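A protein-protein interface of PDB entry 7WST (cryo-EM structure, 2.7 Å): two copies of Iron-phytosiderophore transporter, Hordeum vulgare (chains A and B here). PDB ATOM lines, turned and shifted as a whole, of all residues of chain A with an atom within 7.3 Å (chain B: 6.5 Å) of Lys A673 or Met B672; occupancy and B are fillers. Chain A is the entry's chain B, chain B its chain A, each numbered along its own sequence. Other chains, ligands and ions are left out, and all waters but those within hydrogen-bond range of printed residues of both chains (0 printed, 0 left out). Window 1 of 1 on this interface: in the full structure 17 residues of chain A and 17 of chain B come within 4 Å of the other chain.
Ile A670 touches Leu B675, and with the chains exchanged Leu A675 touches Ile B670.
Cys A671 touches Lys B673, and with the chains exchanged Lys A673 touches Cys B671.
Cys A671 touches Leu B675, and with the chains exchanged Leu A675 touches Cys B671.
Met A672 touches its own counterpart, Met B672.
Positions printed for both chains: 244, 249, 250, 251, 252, 254, 255, 670, 671, 672, 673, 674 and 675.
Of the 22 pairs that touch across the chains among the printed residues, 20 have their exchanged pair printed and touching as well.
The backbone carbonyl oxygen (O) of Tyr B244 is in hydrogen-bond range of the backbone NH (N) of Met B672 (3.2 Å).
N of Gly B246 sits at hydrogen-bond distance from O of Ile B670, at 2.9 Å.
O of Met B672 sits at hydrogen-bond distance from N of Gly B251, 3.0 Å away.
O of Tyr A244 sits at hydrogen-bond distance from N of Met A672 (3.2 Å).
The side-chain sulfur of Cys A250 lies within hydrogen-bond range of the backbone NH of Met A672, at 3.6 Å.
O of Met A672 sits at hydrogen-bond distance from N of Gly A251 (3.0 Å).
Of chain A, only Met A672 (3.8 Å), Lys A673 (3.7 Å) and Phe A674 (3.4 Å) come within 4 Å of Met B672.
Of the printed residues of chain B, Leu A675 touches Ile B670, Cys B671 and Lys B673.
Of the printed residues of chain A, Cys B671 touches Lys A673 (3.6 Å), Phe A674 (3.6 Å) and Leu A675 (2.8 Å).
Gly B251 touches none of the printed residues of chain A.
Gly A251 touches none of the printed residues of chain B.
The nearest residue of chain A that does not touch Met B672 is Phe A255 (4.4 Å).
The backbone carbonyl oxygen (O) of Pro A256 is in hydrogen-bond range of the side-chain hydroxyl (OH) of Tyr B244 (2.5 Å).
O of Leu A675 is in hydrogen-bond range of N of Cys B671, at 2.8 Å.
The backbone carbonyl oxygen of Lys A673 lies within hydrogen-bond range of the backbone NH of Lys B673 (2.9 Å).
The backbone carbonyl oxygen of Leu B675 sits at hydrogen-bond distance from the backbone NH of Cys A671 (2.8 Å).
Printed residues of chain B that touch a printed residue of chain A: Tyr B244, Gly B246, Phe B252, Phe B255, Ile B670, Cys B671, Met B672, Lys B673, Phe B674 and Leu B675.
Hydrophobic or aromatic side chains of chain B that line the printed part of chain A: Tyr B244, Phe B252, Phe B255, Ile B670, Met B672, Phe B674 and Leu B675.
Of the 17 printed residues of chain A, 11 touch a printed residue of chain B.
Hydrophobic or aromatic side chains of chain A within 4 Å of the printed part of chain B: Tyr A244, Phe A252, Phe A255, Ile A670, Met A672, Phe A674, Leu A675 and Ala A677.
Among the printed residues, no Asp or Glu carboxylate lies within 4 Å of a Lys or Arg side-chain nitrogen of the other chain.
Among the printed residues, merely in contact across the chains: Tyr A244 with Phe B255, Phe A252 with Phe B255, Phe A255 with Tyr B244, Phe A255 with Phe B252, Ile A670 with Leu B675, Cys A671 with Lys B673, Cys A671 with Phe B674, Met A672 with Met B672, Met A672 with Lys B673, Met A672 with Phe B674, Lys A673 with Cys B671, Lys A673 with Met B672, Lys A673 with Leu B675, Phe A674 with Cys B671, Phe A674 with Met B672, Leu A675 with Ile B670, Leu A675 with Lys B673 and Ala A677 with Gly B246.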
ATOM      1  N   TYR A 244       6.341 -23.744  10.062  1.00  0.00           N
ATOM      2  CA  TYR A 244       5.575 -23.321   8.901  1.00  0.00           C
ATOM      3  C   TYR A 244       5.387 -21.816   8.827  1.00  0.00           C
ATOM      4  O   TYR A 244       4.737 -21.331   7.896  1.00  0.00           O
ATOM      5  CB  TYR A 244       4.221 -24.034   8.892  1.00  0.00           C
ATOM      6  CG  TYR A 244       4.379 -25.533   8.944  1.00  0.00           C
ATOM      7  CD1 TYR A 244       4.628 -26.260   7.791  1.00  0.00           C
ATOM      8  CD2 TYR A 244       4.322 -26.215  10.151  1.00  0.00           C
ATOM      9  CE1 TYR A 244       4.791 -27.624   7.836  1.00  0.00           C
ATOM     10  CE2 TYR A 244       4.488 -27.579  10.202  1.00  0.00           C
ATOM     11  CZ  TYR A 244       4.723 -28.278   9.041  1.00  0.00           C
ATOM     12  OH  TYR A 244       4.885 -29.638   9.084  1.00  0.00           O
ATOM     13  N   ASP A 248       6.839 -14.127   5.026  1.00  0.00           N
ATOM     14  CA  ASP A 248       6.057 -12.948   5.373  1.00  0.00           C
ATOM     15  C   ASP A 248       4.578 -13.283   5.242  1.00  0.00           C
ATOM     16  O   ASP A 248       4.099 -13.598   4.147  1.00  0.00           O
ATOM     17  CB  ASP A 248       6.446 -11.770   4.483  1.00  0.00           C
ATOM     18  CG  ASP A 248       6.547 -12.152   3.016  1.00  0.00           C
ATOM     19  OD1 ASP A 248       6.459 -13.359   2.702  1.00  0.00           O
ATOM     20  OD2 ASP A 248       6.718 -11.244   2.175  1.00  0.00           O
ATOM     21  N   ALA A 249       3.861 -13.229   6.361  1.00  0.00           N
ATOM     22  CA  ALA A 249       2.418 -13.457   6.404  1.00  0.00           C
ATOM     23  C   ALA A 249       2.053 -14.834   5.849  1.00  0.00           C
ATOM     24  O   ALA A 249       1.353 -14.968   4.845  1.00  0.00           O
ATOM     25  CB  ALA A 249       1.668 -12.348   5.665  1.00  0.00           C
ATOM     26  N   CYS A 250       2.542 -15.869   6.529  1.00  0.00           N
ATOM     27  CA  CYS A 250       2.183 -17.239   6.191  1.00  0.00           C
ATOM     28  C   CYS A 250       2.431 -18.138   7.393  1.00  0.00           C
ATOM     29  O   CYS A 250       3.434 -17.980   8.094  1.00  0.00           O
ATOM     30  CB  CYS A 250       2.962 -17.730   4.963  1.00  0.00           C
ATOM     31  SG  CYS A 250       4.657 -18.290   5.215  1.00  0.00           S
ATOM     32  N   GLY A 251       1.513 -19.061   7.628  1.00  0.00           N
ATOM     33  CA  GLY A 251       1.563 -19.927   8.785  1.00  0.00           C
ATOM     34  C   GLY A 251       0.176 -20.060   9.381  1.00  0.00           C
ATOM     35  O   GLY A 251      -0.801 -19.551   8.842  1.00  0.00           O
ATOM     36  N   PHE A 252       0.107 -20.765  10.511  1.00  0.00           N
ATOM     37  CA  PHE A 252      -1.157 -20.851  11.237  1.00  0.00           C
ATOM     38  C   PHE A 252      -1.547 -19.510  11.835  1.00  0.00           C
ATOM     39  O   PHE A 252      -2.728 -19.274  12.109  1.00  0.00           O
ATOM     40  CB  PHE A 252      -1.072 -21.908  12.337  1.00  0.00           C
ATOM     41  CG  PHE A 252      -1.504 -23.273  11.899  1.00  0.00           C
ATOM     42  CD1 PHE A 252      -2.837 -23.542  11.645  1.00  0.00           C
ATOM     43  CD2 PHE A 252      -0.578 -24.290  11.740  1.00  0.00           C
ATOM     44  CE1 PHE A 252      -3.238 -24.798  11.241  1.00  0.00           C
ATOM     45  CE2 PHE A 252      -0.974 -25.546  11.333  1.00  0.00           C
ATOM     46  CZ  PHE A 252      -2.305 -25.800  11.084  1.00  0.00           C
ATOM     47  N   GLN A 254      -1.267 -16.551  10.317  1.00  0.00           N
ATOM     48  CA  GLN A 254      -1.987 -15.847   9.255  1.00  0.00           C
ATOM     49  C   GLN A 254      -2.978 -16.773   8.549  1.00  0.00           C
ATOM     50  O   GLN A 254      -2.933 -16.958   7.336  1.00  0.00           O
ATOM     51  CB  GLN A 254      -0.996 -15.242   8.267  1.00  0.00           C
ATOM     52  CG  GLN A 254      -0.021 -14.265   8.895  1.00  0.00           C
ATOM     53  CD  GLN A 254      -0.710 -13.054   9.487  1.00  0.00           C
ATOM     54  OE1 GLN A 254      -1.293 -12.245   8.769  1.00  0.00           O
ATOM     55  NE2 GLN A 254      -0.638 -12.918  10.803  1.00  0.00           N
ATOM     56  N   PHE A 255      -3.902 -17.349   9.319  1.00  0.00           N
ATOM     57  CA  PHE A 255      -4.838 -18.327   8.776  1.00  0.00           C
ATOM     58  C   PHE A 255      -6.163 -17.659   8.445  1.00  0.00           C
ATOM     59  O   PHE A 255      -6.840 -17.164   9.359  1.00  0.00           O
ATOM     60  CB  PHE A 255      -5.058 -19.466   9.764  1.00  0.00           C
ATOM     61  CG  PHE A 255      -5.478 -20.759   9.118  1.00  0.00           C
ATOM     62  CD1 PHE A 255      -6.733 -20.894   8.545  1.00  0.00           C
ATOM     63  CD2 PHE A 255      -4.617 -21.845   9.088  1.00  0.00           C
ATOM     64  CE1 PHE A 255      -7.121 -22.078   7.951  1.00  0.00           C
ATOM     65  CE2 PHE A 255      -5.000 -23.033   8.495  1.00  0.00           C
ATOM     66  CZ  PHE A 255      -6.255 -23.147   7.924  1.00  0.00           C
ATOM     67  N   PRO A 256      -6.581 -17.633   7.175  1.00  0.00           N
ATOM     68  CA  PRO A 256      -7.871 -17.025   6.776  1.00  0.00           C
ATOM     69  C   PRO A 256      -9.063 -17.939   7.049  1.00  0.00           C
ATOM     70  O   PRO A 256      -9.619 -18.593   6.173  1.00  0.00           O
ATOM     71  CB  PRO A 256      -7.680 -16.778   5.276  1.00  0.00           C
ATOM     72  CG  PRO A 256      -6.266 -17.178   4.954  1.00  0.00           C
ATOM     73  CD  PRO A 256      -5.835 -18.117   6.010  1.00  0.00           C
ATOM     74  N   TRP A 263      -9.619 -11.789   5.804  1.00  0.00           N
ATOM     75  CA  TRP A 263      -8.277 -11.816   6.372  1.00  0.00           C
ATOM     76  C   TRP A 263      -7.533 -10.514   6.101  1.00  0.00           C
ATOM     77  O   TRP A 263      -6.828 -10.001   6.976  1.00  0.00           O
ATOM     78  CB  TRP A 263      -7.500 -13.012   5.820  1.00  0.00           C
ATOM     79  CG  TRP A 263      -6.064 -13.025   6.221  1.00  0.00           C
ATOM     80  CD1 TRP A 263      -5.556 -13.416   7.420  1.00  0.00           C
ATOM     81  CD2 TRP A 263      -4.945 -12.634   5.419  1.00  0.00           C
ATOM     82  NE1 TRP A 263      -4.193 -13.287   7.423  1.00  0.00           N
ATOM     83  CE2 TRP A 263      -3.791 -12.810   6.203  1.00  0.00           C
ATOM     84  CE3 TRP A 263      -4.809 -12.150   4.115  1.00  0.00           C
ATOM     85  CZ2 TRP A 263      -2.515 -12.523   5.728  1.00  0.00           C
ATOM     86  CZ3 TRP A 263      -3.543 -11.864   3.646  1.00  0.00           C
ATOM     87  CH2 TRP A 263      -2.412 -12.051   4.449  1.00  0.00           C
ATOM     88  N   ILE A 670       9.563 -24.058   6.183  1.00  0.00           N
ATOM     89  CA  ILE A 670       8.401 -24.115   5.307  1.00  0.00           C
ATOM     90  C   ILE A 670       7.559 -22.864   5.509  1.00  0.00           C
ATOM     91  O   ILE A 670       7.545 -22.268   6.590  1.00  0.00           O
ATOM     92  CB  ILE A 670       7.575 -25.396   5.575  1.00  0.00           C
ATOM     93  CG1 ILE A 670       8.478 -26.628   5.509  1.00  0.00           C
ATOM     94  CG2 ILE A 670       6.435 -25.543   4.582  1.00  0.00           C
ATOM     95  CD1 ILE A 670       7.882 -27.866   6.117  1.00  0.00           C
ATOM     96  N   CYS A 671       6.862 -22.457   4.449  1.00  0.00           N
ATOM     97  CA  CYS A 671       5.924 -21.343   4.492  1.00  0.00           C
ATOM     98  C   CYS A 671       4.546 -21.843   4.079  1.00  0.00           C
ATOM     99  O   CYS A 671       4.377 -22.354   2.968  1.00  0.00           O
ATOM    100  CB  CYS A 671       6.392 -20.206   3.580  1.00  0.00           C
ATOM    101  SG  CYS A 671       5.205 -18.864   3.344  1.00  0.00           S
ATOM    102  N   MET A 672       3.568 -21.699   4.972  1.00  0.00           N
ATOM    103  CA  MET A 672       2.185 -22.099   4.705  1.00  0.00           C
ATOM    104  C   MET A 672       1.435 -20.911   4.117  1.00  0.00           C
ATOM    105  O   MET A 672       0.890 -20.074   4.834  1.00  0.00           O
ATOM    106  CB  MET A 672       1.519 -22.610   5.976  1.00  0.00           C
ATOM    107  CG  MET A 672       0.312 -23.491   5.724  1.00  0.00           C
ATOM    108  SD  MET A 672      -0.841 -23.517   7.105  1.00  0.00           S
ATOM    109  CE  MET A 672       0.295 -23.691   8.465  1.00  0.00           C
ATOM    110  N   LYS A 673       1.388 -20.854   2.791  1.00  0.00           N
ATOM    111  CA  LYS A 673       0.804 -19.735   2.071  1.00  0.00           C
ATOM    112  C   LYS A 673      -0.622 -20.062   1.642  1.00  0.00           C
ATOM    113  O   LYS A 673      -0.943 -21.200   1.298  1.00  0.00           O
ATOM    114  CB  LYS A 673       1.657 -19.399   0.846  1.00  0.00           C
ATOM    115  CG  LYS A 673       1.238 -18.158   0.086  1.00  0.00           C
ATOM    116  CD  LYS A 673       1.584 -16.895   0.854  1.00  0.00           C
ATOM    117  CE  LYS A 673       1.301 -15.654   0.026  1.00  0.00           C
ATOM    118  NZ  LYS A 673       1.582 -14.405   0.780  1.00  0.00           N
ATOM    119  N   PHE A 674      -1.481 -19.046   1.671  1.00  0.00           N
ATOM    120  CA  PHE A 674      -2.887 -19.183   1.300  1.00  0.00           C
ATOM    121  C   PHE A 674      -3.139 -18.333   0.062  1.00  0.00           C
ATOM    122  O   PHE A 674      -2.898 -17.122   0.076  1.00  0.00           O
ATOM    123  CB  PHE A 674      -3.802 -18.766   2.450  1.00  0.00           C
ATOM    124  CG  PHE A 674      -3.654 -19.613   3.679  1.00  0.00           C
ATOM    125  CD1 PHE A 674      -2.652 -19.354   4.600  1.00  0.00           C
ATOM    126  CD2 PHE A 674      -4.518 -20.665   3.920  1.00  0.00           C
ATOM    127  CE1 PHE A 674      -2.515 -20.129   5.731  1.00  0.00           C
ATOM    128  CE2 PHE A 674      -4.387 -21.439   5.052  1.00  0.00           C
ATOM    129  CZ  PHE A 674      -3.381 -21.174   5.955  1.00  0.00           C
ATOM    130  N   LEU A 675      -3.626 -18.965  -1.000  1.00  0.00           N
ATOM    131  CA  LEU A 675      -3.835 -18.301  -2.275  1.00  0.00           C
ATOM    132  C   LEU A 675      -5.288 -18.435  -2.720  1.00  0.00           C
ATOM    133  O   LEU A 675      -5.981 -19.373  -2.315  1.00  0.00           O
ATOM    134  CB  LEU A 675      -2.916 -18.888  -3.353  1.00  0.00           C
ATOM    135  CG  LEU A 675      -1.414 -18.794  -3.086  1.00  0.00           C
ATOM    136  CD1 LEU A 675      -0.888 -20.099  -2.521  1.00  0.00           C
ATOM    137  CD2 LEU A 675      -0.668 -18.417  -4.351  1.00  0.00           C
ATOM    138  N   ALA A 677      -6.988 -19.773  -4.957  1.00  0.00           N
ATOM    139  CA  ALA A 677      -7.207 -20.856  -5.918  1.00  0.00           C
ATOM    140  C   ALA A 677      -6.754 -20.458  -7.319  1.00  0.00           C
ATOM    141  O   ALA A 677      -7.433 -20.718  -8.315  1.00  0.00           O
ATOM    142  CB  ALA A 677      -8.670 -21.299  -5.923  1.00  0.00           C
ATOM    143  N   GLN B 241     -12.308 -28.354   5.972  1.00  0.00           N
ATOM    144  CA  GLN B 241     -11.180 -28.657   5.096  1.00  0.00           C
ATOM    145  C   GLN B 241     -11.475 -28.321   3.643  1.00  0.00           C
ATOM    146  O   GLN B 241     -10.557 -27.987   2.887  1.00  0.00           O
ATOM    147  CB  GLN B 241     -10.821 -30.134   5.199  1.00  0.00           C
ATOM    148  CG  GLN B 241     -10.092 -30.541   6.444  1.00  0.00           C
ATOM    149  CD  GLN B 241      -9.627 -31.971   6.363  1.00  0.00           C
ATOM    150  OE1 GLN B 241      -8.675 -32.286   5.651  1.00  0.00           O
ATOM    151  NE2 GLN B 241     -10.318 -32.857   7.064  1.00  0.00           N
ATOM    152  N   TYR B 244     -10.217 -25.128   1.555  1.00  0.00           N
ATOM    153  CA  TYR B 244      -8.800 -24.883   1.340  1.00  0.00           C
ATOM    154  C   TYR B 244      -8.148 -25.913   0.434  1.00  0.00           C
ATOM    155  O   TYR B 244      -6.941 -25.827   0.189  1.00  0.00           O
ATOM    156  CB  TYR B 244      -8.080 -24.821   2.690  1.00  0.00           C
ATOM    157  CG  TYR B 244      -8.695 -23.790   3.603  1.00  0.00           C
ATOM    158  CD1 TYR B 244      -8.349 -22.453   3.498  1.00  0.00           C
ATOM    159  CD2 TYR B 244      -9.652 -24.149   4.541  1.00  0.00           C
ATOM    160  CE1 TYR B 244      -8.920 -21.507   4.315  1.00  0.00           C
ATOM    161  CE2 TYR B 244     -10.230 -23.206   5.359  1.00  0.00           C
ATOM    162  CZ  TYR B 244      -9.860 -21.887   5.241  1.00  0.00           C
ATOM    163  OH  TYR B 244     -10.427 -20.943   6.056  1.00  0.00           O
ATOM    164  N   THR B 245      -8.906 -26.884  -0.065  1.00  0.00           N
ATOM    165  CA  THR B 245      -8.420 -27.821  -1.075  1.00  0.00           C
ATOM    166  C   THR B 245      -8.756 -27.332  -2.479  1.00  0.00           C
ATOM    167  O   THR B 245      -9.306 -28.062  -3.300  1.00  0.00           O
ATOM    168  CB  THR B 245      -9.006 -29.203  -0.822  1.00  0.00           C
ATOM    169  OG1 THR B 245     -10.435 -29.115  -0.792  1.00  0.00           O
ATOM    170  CG2 THR B 245      -8.518 -29.748   0.503  1.00  0.00           C
ATOM    171  N   GLY B 246      -8.404 -26.084  -2.765  1.00  0.00           N
ATOM    172  CA  GLY B 246      -8.768 -25.462  -4.021  1.00  0.00           C
ATOM    173  C   GLY B 246      -7.639 -25.420  -5.024  1.00  0.00           C
ATOM    174  O   GLY B 246      -7.460 -24.422  -5.726  1.00  0.00           O
ATOM    175  N   GLY B 247      -6.870 -26.497  -5.101  1.00  0.00           N
ATOM    176  CA  GLY B 247      -5.784 -26.558  -6.058  1.00  0.00           C
ATOM    177  C   GLY B 247      -5.204 -27.950  -6.101  1.00  0.00           C
ATOM    178  O   GLY B 247      -5.582 -28.834  -5.327  1.00  0.00           O
ATOM    179  N   ALA B 249      -2.789 -30.570  -5.199  1.00  0.00           N
ATOM    180  CA  ALA B 249      -1.889 -30.899  -4.096  1.00  0.00           C
ATOM    181  C   ALA B 249      -1.709 -29.712  -3.149  1.00  0.00           C
ATOM    182  O   ALA B 249      -0.614 -29.173  -2.978  1.00  0.00           O
ATOM    183  CB  ALA B 249      -0.540 -31.395  -4.621  1.00  0.00           C
ATOM    184  N   CYS B 250      -2.815 -29.309  -2.526  1.00  0.00           N
ATOM    185  CA  CYS B 250      -2.777 -28.269  -1.507  1.00  0.00           C
ATOM    186  C   CYS B 250      -4.012 -28.381  -0.625  1.00  0.00           C
ATOM    187  O   CYS B 250      -5.112 -28.639  -1.121  1.00  0.00           O
ATOM    188  CB  CYS B 250      -2.676 -26.875  -2.141  1.00  0.00           C
ATOM    189  SG  CYS B 250      -4.190 -26.130  -2.775  1.00  0.00           S
ATOM    190  N   GLY B 251      -3.818 -28.201   0.671  1.00  0.00           N
ATOM    191  CA  GLY B 251      -4.876 -28.368   1.643  1.00  0.00           C
ATOM    192  C   GLY B 251      -4.343 -29.110   2.852  1.00  0.00           C
ATOM    193  O   GLY B 251      -3.156 -29.405   2.947  1.00  0.00           O
ATOM    194  N   PHE B 252      -5.250 -29.406   3.784  1.00  0.00           N
ATOM    195  CA  PHE B 252      -4.872 -30.228   4.930  1.00  0.00           C
ATOM    196  C   PHE B 252      -4.567 -31.657   4.512  1.00  0.00           C
ATOM    197  O   PHE B 252      -3.852 -32.370   5.223  1.00  0.00           O
ATOM    198  CB  PHE B 252      -5.977 -30.216   5.985  1.00  0.00           C
ATOM    199  CG  PHE B 252      -5.823 -29.136   7.011  1.00  0.00           C
ATOM    200  CD1 PHE B 252      -4.819 -29.205   7.960  1.00  0.00           C
ATOM    201  CD2 PHE B 252      -6.681 -28.051   7.027  1.00  0.00           C
ATOM    202  CE1 PHE B 252      -4.674 -28.212   8.905  1.00  0.00           C
ATOM    203  CE2 PHE B 252      -6.538 -27.054   7.969  1.00  0.00           C
ATOM    204  CZ  PHE B 252      -5.534 -27.135   8.909  1.00  0.00           C
ATOM    205  N   VAL B 253      -5.104 -32.094   3.373  1.00  0.00           N
ATOM    206  CA  VAL B 253      -4.844 -33.447   2.901  1.00  0.00           C
ATOM    207  C   VAL B 253      -3.395 -33.588   2.445  1.00  0.00           C
ATOM    208  O   VAL B 253      -2.765 -34.629   2.657  1.00  0.00           O
ATOM    209  CB  VAL B 253      -5.852 -33.824   1.796  1.00  0.00           C
ATOM    210  CG1 VAL B 253      -5.831 -32.806   0.662  1.00  0.00           C
ATOM    211  CG2 VAL B 253      -5.599 -35.232   1.285  1.00  0.00           C
ATOM    212  N   GLN B 254      -2.846 -32.564   1.802  1.00  0.00           N
ATOM    213  CA  GLN B 254      -1.436 -32.562   1.407  1.00  0.00           C
ATOM    214  C   GLN B 254      -0.584 -31.776   2.404  1.00  0.00           C
ATOM    215  O   GLN B 254       0.114 -30.830   2.048  1.00  0.00           O
ATOM    216  CB  GLN B 254      -1.293 -32.003  -0.005  1.00  0.00           C
ATOM    217  CG  GLN B 254      -2.068 -32.775  -1.053  1.00  0.00           C
ATOM    218  CD  GLN B 254      -1.594 -34.206  -1.193  1.00  0.00           C
ATOM    219  OE1 GLN B 254      -0.469 -34.460  -1.618  1.00  0.00           O
ATOM    220  NE2 GLN B 254      -2.454 -35.150  -0.842  1.00  0.00           N
ATOM    221  N   PHE B 255      -0.623 -32.189   3.672  1.00  0.00           N
ATOM    222  CA  PHE B 255       0.070 -31.459   4.727  1.00  0.00           C
ATOM    223  C   PHE B 255       1.413 -32.110   5.019  1.00  0.00           C
ATOM    224  O   PHE B 255       1.445 -33.265   5.468  1.00  0.00           O
ATOM    225  CB  PHE B 255      -0.777 -31.415   5.993  1.00  0.00           C
ATOM    226  CG  PHE B 255      -0.474 -30.241   6.886  1.00  0.00           C
ATOM    227  CD1 PHE B 255       0.726 -30.163   7.577  1.00  0.00           C
ATOM    228  CD2 PHE B 255      -1.392 -29.215   7.039  1.00  0.00           C
ATOM    229  CE1 PHE B 255       1.007 -29.089   8.396  1.00  0.00           C
ATOM    230  CE2 PHE B 255      -1.116 -28.136   7.857  1.00  0.00           C
ATOM    231  CZ  PHE B 255       0.087 -28.074   8.535  1.00  0.00           C
ATOM    232  N   ILE B 670     -10.033 -21.322  -1.763  1.00  0.00           N
ATOM    233  CA  ILE B 670      -8.678 -21.067  -1.295  1.00  0.00           C
ATOM    234  C   ILE B 670      -7.831 -22.313  -1.506  1.00  0.00           C
ATOM    235  O   ILE B 670      -8.335 -23.440  -1.494  1.00  0.00           O
ATOM    236  CB  ILE B 670      -8.682 -20.636   0.191  1.00  0.00           C
ATOM    237  CG1 ILE B 670      -9.654 -19.474   0.399  1.00  0.00           C
ATOM    238  CG2 ILE B 670      -7.295 -20.236   0.661  1.00  0.00           C
ATOM    239  CD1 ILE B 670     -10.024 -19.226   1.835  1.00  0.00           C
ATOM    240  N   CYS B 671      -6.533 -22.104  -1.718  1.00  0.00           N
ATOM    241  CA  CYS B 671      -5.560 -23.182  -1.835  1.00  0.00           C
ATOM    242  C   CYS B 671      -4.494 -23.002  -0.762  1.00  0.00           C
ATOM    243  O   CYS B 671      -3.818 -21.971  -0.724  1.00  0.00           O
ATOM    244  CB  CYS B 671      -4.936 -23.199  -3.232  1.00  0.00           C
ATOM    245  SG  CYS B 671      -3.537 -24.325  -3.442  1.00  0.00           S
ATOM    246  N   MET B 672      -4.351 -24.001   0.107  1.00  0.00           N
ATOM    247  CA  MET B 672      -3.345 -23.989   1.171  1.00  0.00           C
ATOM    248  C   MET B 672      -2.069 -24.638   0.651  1.00  0.00           C
ATOM    249  O   MET B 672      -1.893 -25.853   0.713  1.00  0.00           O
ATOM    250  CB  MET B 672      -3.867 -24.697   2.414  1.00  0.00           C
ATOM    251  CG  MET B 672      -3.145 -24.312   3.690  1.00  0.00           C
ATOM    252  SD  MET B 672      -3.250 -25.576   4.967  1.00  0.00           S
ATOM    253  CE  MET B 672      -4.975 -26.002   4.849  1.00  0.00           C
ATOM    254  N   LYS B 673      -1.159 -23.809   0.152  1.00  0.00           N
ATOM    255  CA  LYS B 673       0.065 -24.272  -0.480  1.00  0.00           C
ATOM    256  C   LYS B 673       1.228 -24.214   0.503  1.00  0.00           C
ATOM    257  O   LYS B 673       1.316 -23.316   1.341  1.00  0.00           O
ATOM    258  CB  LYS B 673       0.374 -23.418  -1.711  1.00  0.00           C
ATOM    259  CG  LYS B 673       1.548 -23.884  -2.546  1.00  0.00           C
ATOM    260  CD  LYS B 673       1.207 -25.142  -3.325  1.00  0.00           C
ATOM    261  CE  LYS B 673       2.331 -25.521  -4.273  1.00  0.00           C
ATOM    262  NZ  LYS B 673       2.040 -26.780  -5.007  1.00  0.00           N
ATOM    263  N   PHE B 674       2.125 -25.192   0.395  1.00  0.00           N
ATOM    264  CA  PHE B 674       3.297 -25.296   1.261  1.00  0.00           C
ATOM    265  C   PHE B 674       4.542 -25.127   0.401  1.00  0.00           C
ATOM    266  O   PHE B 674       4.747 -25.880  -0.555  1.00  0.00           O
ATOM    267  CB  PHE B 674       3.317 -26.629   2.002  1.00  0.00           C
ATOM    268  CG  PHE B 674       2.150 -26.828   2.926  1.00  0.00           C
ATOM    269  CD1 PHE B 674       0.940 -27.300   2.445  1.00  0.00           C
ATOM    270  CD2 PHE B 674       2.262 -26.546   4.275  1.00  0.00           C
ATOM    271  CE1 PHE B 674      -0.132 -27.484   3.291  1.00  0.00           C
ATOM    272  CE2 PHE B 674       1.194 -26.733   5.124  1.00  0.00           C
ATOM    273  CZ  PHE B 674      -0.006 -27.197   4.630  1.00  0.00           C
ATOM    274  N   LEU B 675       5.369 -24.146   0.743  1.00  0.00           N
ATOM    275  CA  LEU B 675       6.549 -23.814  -0.036  1.00  0.00           C
ATOM    276  C   LEU B 675       7.803 -23.884   0.832  1.00  0.00           C
ATOM    277  O   LEU B 675       7.726 -23.737   2.054  1.00  0.00           O
ATOM    278  CB  LEU B 675       6.427 -22.411  -0.641  1.00  0.00           C
ATOM    279  CG  LEU B 675       5.243 -22.179  -1.579  1.00  0.00           C
ATOM    280  CD1 LEU B 675       4.101 -21.505  -0.842  1.00  0.00           C
ATOM    281  CD2 LEU B 675       5.665 -21.359  -2.782  1.00  0.00           C
